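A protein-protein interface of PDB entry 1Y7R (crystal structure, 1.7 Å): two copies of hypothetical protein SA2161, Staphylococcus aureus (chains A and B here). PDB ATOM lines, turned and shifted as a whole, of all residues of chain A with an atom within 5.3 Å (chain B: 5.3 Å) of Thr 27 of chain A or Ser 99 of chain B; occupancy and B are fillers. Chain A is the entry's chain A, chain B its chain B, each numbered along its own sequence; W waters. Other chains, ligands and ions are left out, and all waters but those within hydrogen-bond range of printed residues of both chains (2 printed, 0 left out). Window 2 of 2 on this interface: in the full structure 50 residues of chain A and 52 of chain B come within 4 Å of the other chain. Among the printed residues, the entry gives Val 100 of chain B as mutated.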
ATOM      1  N   CYS A  15      24.037 -24.476  -4.528  1.00  0.00           N
ATOM      2  CA  CYS A  15      24.000 -23.091  -4.947  1.00  0.00           C
ATOM      3  C   CYS A  15      24.569 -22.980  -6.369  1.00  0.00           C
ATOM      4  O   CYS A  15      24.031 -22.244  -7.217  1.00  0.00           O
ATOM      5  CB  CYS A  15      24.820 -22.245  -3.974  1.00  0.00           C
ATOM      6  SG  CYS A  15      23.985 -22.074  -2.371  1.00  0.00           S
ATOM      7  N   PRO A  25      19.770 -17.171  -7.629  1.00  0.00           N
ATOM      8  CA  PRO A  25      20.601 -17.808  -6.605  1.00  0.00           C
ATOM      9  C   PRO A  25      19.900 -17.962  -5.257  1.00  0.00           C
ATOM     10  O   PRO A  25      18.922 -17.225  -4.947  1.00  0.00           O
ATOM     11  CB  PRO A  25      21.795 -16.834  -6.461  1.00  0.00           C
ATOM     12  CG  PRO A  25      21.220 -15.509  -6.840  1.00  0.00           C
ATOM     13  CD  PRO A  25      20.228 -15.806  -7.942  1.00  0.00           C
ATOM     14  N   LYS A  26      20.370 -18.934  -4.481  1.00  0.00           N
ATOM     15  CA  LYS A  26      20.007 -19.023  -3.069  1.00  0.00           C
ATOM     16  C   LYS A  26      21.254 -18.703  -2.274  1.00  0.00           C
ATOM     17  O   LYS A  26      22.351 -19.097  -2.657  1.00  0.00           O
ATOM     18  CB  LYS A  26      19.542 -20.427  -2.669  1.00  0.00           C
ATOM     19  CG  LYS A  26      18.231 -20.872  -3.217  1.00  0.00           C
ATOM     20  CD  LYS A  26      17.036 -20.035  -2.792  1.00  0.00           C
ATOM     21  CE  LYS A  26      15.813 -20.594  -3.487  1.00  0.00           C
ATOM     22  NZ  LYS A  26      14.536 -19.874  -3.216  1.00  0.00           N
ATOM     23  N   THR A  27      21.083 -18.016  -1.146  1.00  0.00           N
ATOM     24  CA  THR A  27      22.231 -17.727  -0.292  1.00  0.00           C
ATOM     25  C   THR A  27      22.684 -19.023   0.339  1.00  0.00           C
ATOM     26  O   THR A  27      21.890 -19.946   0.513  1.00  0.00           O
ATOM     27  CB  THR A  27      21.887 -16.725   0.820  1.00  0.00           C
ATOM     28  OG1 THR A  27      20.902 -17.306   1.677  1.00  0.00           O
ATOM     29  CG2 THR A  27      21.321 -15.435   0.217  1.00  0.00           C
ATOM     30  N   ARG A  28      23.957 -19.092   0.701  1.00  0.00           N
ATOM     31  CA  ARG A  28      24.433 -20.266   1.408  1.00  0.00           C
ATOM     32  C   ARG A  28      23.714 -20.472   2.748  1.00  0.00           C
ATOM     33  O   ARG A  28      23.498 -21.629   3.165  1.00  0.00           O
ATOM     34  CB  ARG A  28      25.965 -20.269   1.515  1.00  0.00           C
ATOM     35  CG  ARG A  28      26.616 -20.580   0.166  1.00  0.00           C
ATOM     36  CD  ARG A  28      28.125 -20.576   0.273  1.00  0.00           C
ATOM     37  NE  ARG A  28      28.635 -19.229   0.494  1.00  0.00           N
ATOM     38  CZ  ARG A  28      29.656 -18.725  -0.186  1.00  0.00           C
ATOM     39  NH1 ARG A  28      30.093 -17.491   0.041  1.00  0.00           N
ATOM     40  NH2 ARG A  28      30.246 -19.475  -1.103  1.00  0.00           N
ATOM     41  N   GLU A  29      23.324 -19.371   3.407  1.00  0.00           N
ATOM     42  CA  GLU A  29      22.525 -19.467   4.621  1.00  0.00           C
ATOM     43  C   GLU A  29      21.189 -20.174   4.357  1.00  0.00           C
ATOM     44  O   GLU A  29      20.753 -21.038   5.149  1.00  0.00           O
ATOM     45  CB  GLU A  29      22.261 -18.106   5.259  1.00  0.00           C
ATOM     46  CG  GLU A  29      21.599 -18.190   6.659  1.00  0.00           C
ATOM     47  CD  GLU A  29      20.914 -16.896   7.136  1.00  0.00           C
ATOM     48  OE1 GLU A  29      20.664 -15.976   6.314  1.00  0.00           O
ATOM     49  OE2 GLU A  29      20.608 -16.799   8.353  1.00  0.00           O
ATOM     50  N   ALA A  30      20.509 -19.805   3.265  1.00  0.00           N
ATOM     51  CA  ALA A  30      19.217 -20.460   3.010  1.00  0.00           C
ATOM     52  C   ALA A  30      19.435 -21.940   2.705  1.00  0.00           C
ATOM     53  O   ALA A  30      18.671 -22.803   3.176  1.00  0.00           O
ATOM     54  CB  ALA A  30      18.435 -19.779   1.862  1.00  0.00           C
ATOM     55  N   ALA A  31      20.471 -22.224   1.910  1.00  0.00           N
ATOM     56  CA  ALA A  31      20.788 -23.593   1.533  1.00  0.00           C
ATOM     57  C   ALA A  31      21.105 -24.454   2.763  1.00  0.00           C
ATOM     58  O   ALA A  31      20.642 -25.590   2.885  1.00  0.00           O
ATOM     59  CB  ALA A  31      21.930 -23.590   0.529  1.00  0.00           C
ATOM     60  N   GLU A  32      21.875 -23.898   3.690  1.00  0.00           N
ATOM     61  CA  GLU A  32      22.254 -24.606   4.910  1.00  0.00           C
ATOM     62  C   GLU A  32      21.008 -24.978   5.695  1.00  0.00           C
ATOM     63  O   GLU A  32      20.876 -26.106   6.169  1.00  0.00           O
ATOM     64  CB  GLU A  32      23.122 -23.714   5.782  1.00  0.00           C
ATOM     65  CG  GLU A  32      24.571 -23.624   5.359  1.00  0.00           C
ATOM     66  CD  GLU A  32      25.419 -22.844   6.346  1.00  0.00           C
ATOM     67  OE1 GLU A  32      24.929 -21.844   6.927  1.00  0.00           O
ATOM     68  OE2 GLU A  32      26.596 -23.224   6.542  1.00  0.00           O
ATOM     69  N   LYS A 132       9.077 -13.370  -2.426  1.00  0.00           N
ATOM     70  CA  LYS A 132      10.482 -13.729  -2.361  1.00  0.00           C
ATOM     71  C   LYS A 132      11.192 -12.776  -1.412  1.00  0.00           C
ATOM     72  O   LYS A 132      11.049 -11.549  -1.535  1.00  0.00           O
ATOM     73  CB  LYS A 132      11.102 -13.689  -3.754  1.00  0.00           C
ATOM     74  CG  LYS A 132      12.597 -13.950  -3.728  1.00  0.00           C
ATOM     75  CD  LYS A 132      12.998 -14.851  -4.804  1.00  0.00           C
ATOM     76  CE  LYS A 132      14.490 -15.022  -4.734  1.00  0.00           C
ATOM     77  NZ  LYS A 132      15.007 -15.035  -6.114  1.00  0.00           N
ATOM     78  N   TYR A 133      11.904 -13.347  -0.440  1.00  0.00           N
ATOM     79  CA  TYR A 133      12.623 -12.556   0.556  1.00  0.00           C
ATOM     80  C   TYR A 133      14.064 -12.246   0.172  1.00  0.00           C
ATOM     81  O   TYR A 133      14.644 -11.269   0.689  1.00  0.00           O
ATOM     82  CB  TYR A 133      12.582 -13.249   1.904  1.00  0.00           C
ATOM     83  CG  TYR A 133      11.203 -13.252   2.530  1.00  0.00           C
ATOM     84  CD1 TYR A 133      10.631 -12.075   3.020  1.00  0.00           C
ATOM     85  CD2 TYR A 133      10.473 -14.427   2.624  1.00  0.00           C
ATOM     86  CE1 TYR A 133       9.358 -12.081   3.593  1.00  0.00           C
ATOM     87  CE2 TYR A 133       9.205 -14.455   3.204  1.00  0.00           C
ATOM     88  CZ  TYR A 133       8.655 -13.282   3.685  1.00  0.00           C
ATOM     89  OH  TYR A 133       7.405 -13.330   4.257  1.00  0.00           O
ATOM     90  N   THR B  62      14.779 -22.617   2.182  1.00  0.00           N
ATOM     91  CA  THR B  62      14.919 -22.230   0.820  1.00  0.00           C
ATOM     92  C   THR B  62      13.515 -22.029   0.200  1.00  0.00           C
ATOM     93  O   THR B  62      13.318 -21.177  -0.674  1.00  0.00           O
ATOM     94  CB  THR B  62      15.677 -23.414   0.229  1.00  0.00           C
ATOM     95  OG1 THR B  62      17.053 -23.109  -0.073  1.00  0.00           O
ATOM     96  CG2 THR B  62      14.894 -24.190  -0.763  1.00  0.00           C
ATOM     97  N   VAL B  97      14.790 -16.347   5.395  1.00  0.00           N
ATOM     98  CA  VAL B  97      15.996 -15.534   5.257  1.00  0.00           C
ATOM     99  C   VAL B  97      16.030 -14.949   3.845  1.00  0.00           C
ATOM    100  O   VAL B  97      15.146 -15.239   3.039  1.00  0.00           O
ATOM    101  CB  VAL B  97      17.266 -16.364   5.556  1.00  0.00           C
ATOM    102  CG1 VAL B  97      17.243 -16.857   7.001  1.00  0.00           C
ATOM    103  CG2 VAL B  97      17.411 -17.516   4.581  1.00  0.00           C
ATOM    104  N   GLU B  98      17.034 -14.122   3.538  1.00  0.00           N
ATOM    105  CA  GLU B  98      17.156 -13.595   2.179  1.00  0.00           C
ATOM    106  C   GLU B  98      17.273 -14.764   1.214  1.00  0.00           C
ATOM    107  O   GLU B  98      18.027 -15.682   1.484  1.00  0.00           O
ATOM    108  CB  GLU B  98      18.360 -12.672   2.058  1.00  0.00           C
ATOM    109  CG  GLU B  98      18.002 -11.282   2.541  1.00  0.00           C
ATOM    110  CD  GLU B  98      19.096 -10.265   2.298  1.00  0.00           C
ATOM    111  OE1 GLU B  98      20.078 -10.604   1.592  1.00  0.00           O
ATOM    112  OE2 GLU B  98      18.962  -9.133   2.834  1.00  0.00           O
ATOM    113  N   SER B  99      16.482 -14.704   0.136  1.00  0.00           N
ATOM    114  CA  SER B  99      16.406 -15.679  -0.962  1.00  0.00           C
ATOM    115  C   SER B  99      15.330 -16.747  -0.733  1.00  0.00           C
ATOM    116  O   SER B  99      15.006 -17.481  -1.657  1.00  0.00           O
ATOM    117  CB  SER B  99      17.785 -16.288  -1.343  1.00  0.00           C
ATOM    118  OG  SER B  99      18.174 -17.363  -0.485  1.00  0.00           O
ATOM    119  N   VAL B 100      14.786 -16.837   0.490  1.00  0.00           N
ATOM    120  CA  VAL B 100      13.645 -17.757   0.715  1.00  0.00           C
ATOM    121  C   VAL B 100      12.475 -17.437  -0.228  1.00  0.00           C
ATOM    122  O   VAL B 100      12.108 -16.254  -0.412  1.00  0.00           O
ATOM    123  CB  VAL B 100      13.136 -17.684   2.142  1.00  0.00           C
ATOM    124  CG1 VAL B 100      11.922 -18.610   2.296  1.00  0.00           C
ATOM    125  CG2 VAL B 100      14.221 -18.055   3.100  1.00  0.00           C
ATOM    126  N   TYR B 101      11.878 -18.487  -0.797  1.00  0.00           N
ATOM    127  CA  TYR B 101      10.738 -18.312  -1.681  1.00  0.00           C
ATOM    128  C   TYR B 101       9.524 -18.934  -0.992  1.00  0.00           C
ATOM    129  O   TYR B 101       9.632 -20.010  -0.386  1.00  0.00           O
ATOM    130  CB  TYR B 101      11.050 -19.055  -2.967  1.00  0.00           C
ATOM    131  CG  TYR B 101      10.002 -19.030  -4.062  1.00  0.00           C
ATOM    132  CD1 TYR B 101       9.989 -17.999  -4.991  1.00  0.00           C
ATOM    133  CD2 TYR B 101       9.075 -20.063  -4.201  1.00  0.00           C
ATOM    134  CE1 TYR B 101       9.066 -17.977  -6.057  1.00  0.00           C
ATOM    135  CE2 TYR B 101       8.141 -20.056  -5.255  1.00  0.00           C
ATOM    136  CZ  TYR B 101       8.137 -19.017  -6.167  1.00  0.00           C
ATOM    137  OH  TYR B 101       7.223 -18.993  -7.205  1.00  0.00           O
HETATM  138  O   HOH W   1      18.960 -13.301   5.756  1.00  0.00           O
HETATM  139  O   HOH W   2      20.035 -15.644   3.454  1.00  0.00           O
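O of Thr 62 of chain B sits at hydrogen-bond distance from NZ of Lys 26 of chain A (3.1 Å).
The backbone NH (N) of Thr 27 of chain A sits at hydrogen-bond distance from the side-chain hydroxyl (OG) of Ser 99 of chain B, at 3.1 Å.
O of Glu 98 of chain B is in hydrogen-bond range of OG1 of Thr 27 of chain A, 3.3 Å away.
The side-chain amino group (NZ) of Lys 26 of chain A sits at hydrogen-bond distance from the backbone carbonyl oxygen (O) of Ser 99 of chain B (2.9 Å).
The backbone NH of Tyr 133 of chain A is in hydrogen-bond range of the backbone carbonyl oxygen of Val 100 of chain B (2.9 Å).
The side-chain hydroxyl (OG1) of Thr 27 of chain A is in hydrogen-bond range of the backbone NH (N) of Ala 30 of chain A (3.0 Å).
O of Thr 62 of chain B sits at hydrogen-bond distance from N of Tyr 101 of chain B, at 3.1 Å.
The backbone carbonyl oxygen (O) of Lys 26 of chain A is in hydrogen-bond range of the side-chain sulfur (SG) of Cys 15 of chain A, 3.4 Å away.
Among the printed residues, pairs that only touch across the chains: Ala 30 of chain A with Ser 99 of chain B (3.4 Å), Tyr 133 of chain A with Val 97 of chain B (3.4 Å), Tyr 133 of chain A with Ser 99 of chain B (3.4 Å), Glu 29 of chain A with Val 97 of chain B (3.5 Å), Lys 132 of chain A with Val 100 of chain B (3.6 Å), Lys 26 of chain A with Tyr 101 of chain B (3.6 Å), Ala 30 of chain A with Thr 62 of chain B (3.6 Å), Ala 30 of chain A with Val 97 of chain B (3.7 Å), Tyr 133 of chain A with Glu 98 of chain B (3.7 Å), Pro 25 of chain A with Ser 99 of chain B (3.9 Å) and Lys 132 of chain A with Ser 99 of chain B (3.97 Å).
Of chain B, only Glu 98 (3.3 Å) and Ser 99 (3.1 Å) come within 4 Å of Thr 27 of chain A.
Printed residues of chain A within 4 Å of Ser 99 of chain B: Pro 25, Lys 26, Thr 27, Ala 30, Lys 132 and Tyr 133.
Of the printed residues of chain A, Val 97 of chain B touches Glu 29, Ala 30 and Tyr 133.
Printed residues of chain B within 4 Å of Lys 132 of chain A: Ser 99 (3.97 Å) and Val 100 (3.6 Å).
Printed residues of chain B within 4 Å of Tyr 133 of chain A: Val 97 (3.4 Å), Glu 98 (3.7 Å), Ser 99 (3.4 Å) and Val 100 (2.9 Å).
Cys 15 of chain A touches none of the printed residues of chain B.
Arg 28 of chain A touches none of the printed residues of chain B.
The nearest printed residue of chain B that does not touch Ala 30 of chain A is Glu 98 of chain B (4.1 Å).
Printed residues of chain B that touch a printed residue of chain A: Thr 62, Val 97, Glu 98, Ser 99, Val 100 and Tyr 101.
Hydrophobic or aromatic side chains of chain B that line the printed part of chain A: Val 97 and Tyr 101.
No position is printed for both chains.
Water W2 lies within hydrogen-bond range of the side-chain hydroxyl of Thr 27 of chain A, the backbone carbonyl oxygen of Glu 98 of chain B and the side-chain carboxylate of Glu 29 of chain A.
Water W1 lies within hydrogen-bond range of N of Glu 98 of chain B (3.1 Å) and OE1 of Glu 29 of chain A (3.2 Å).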
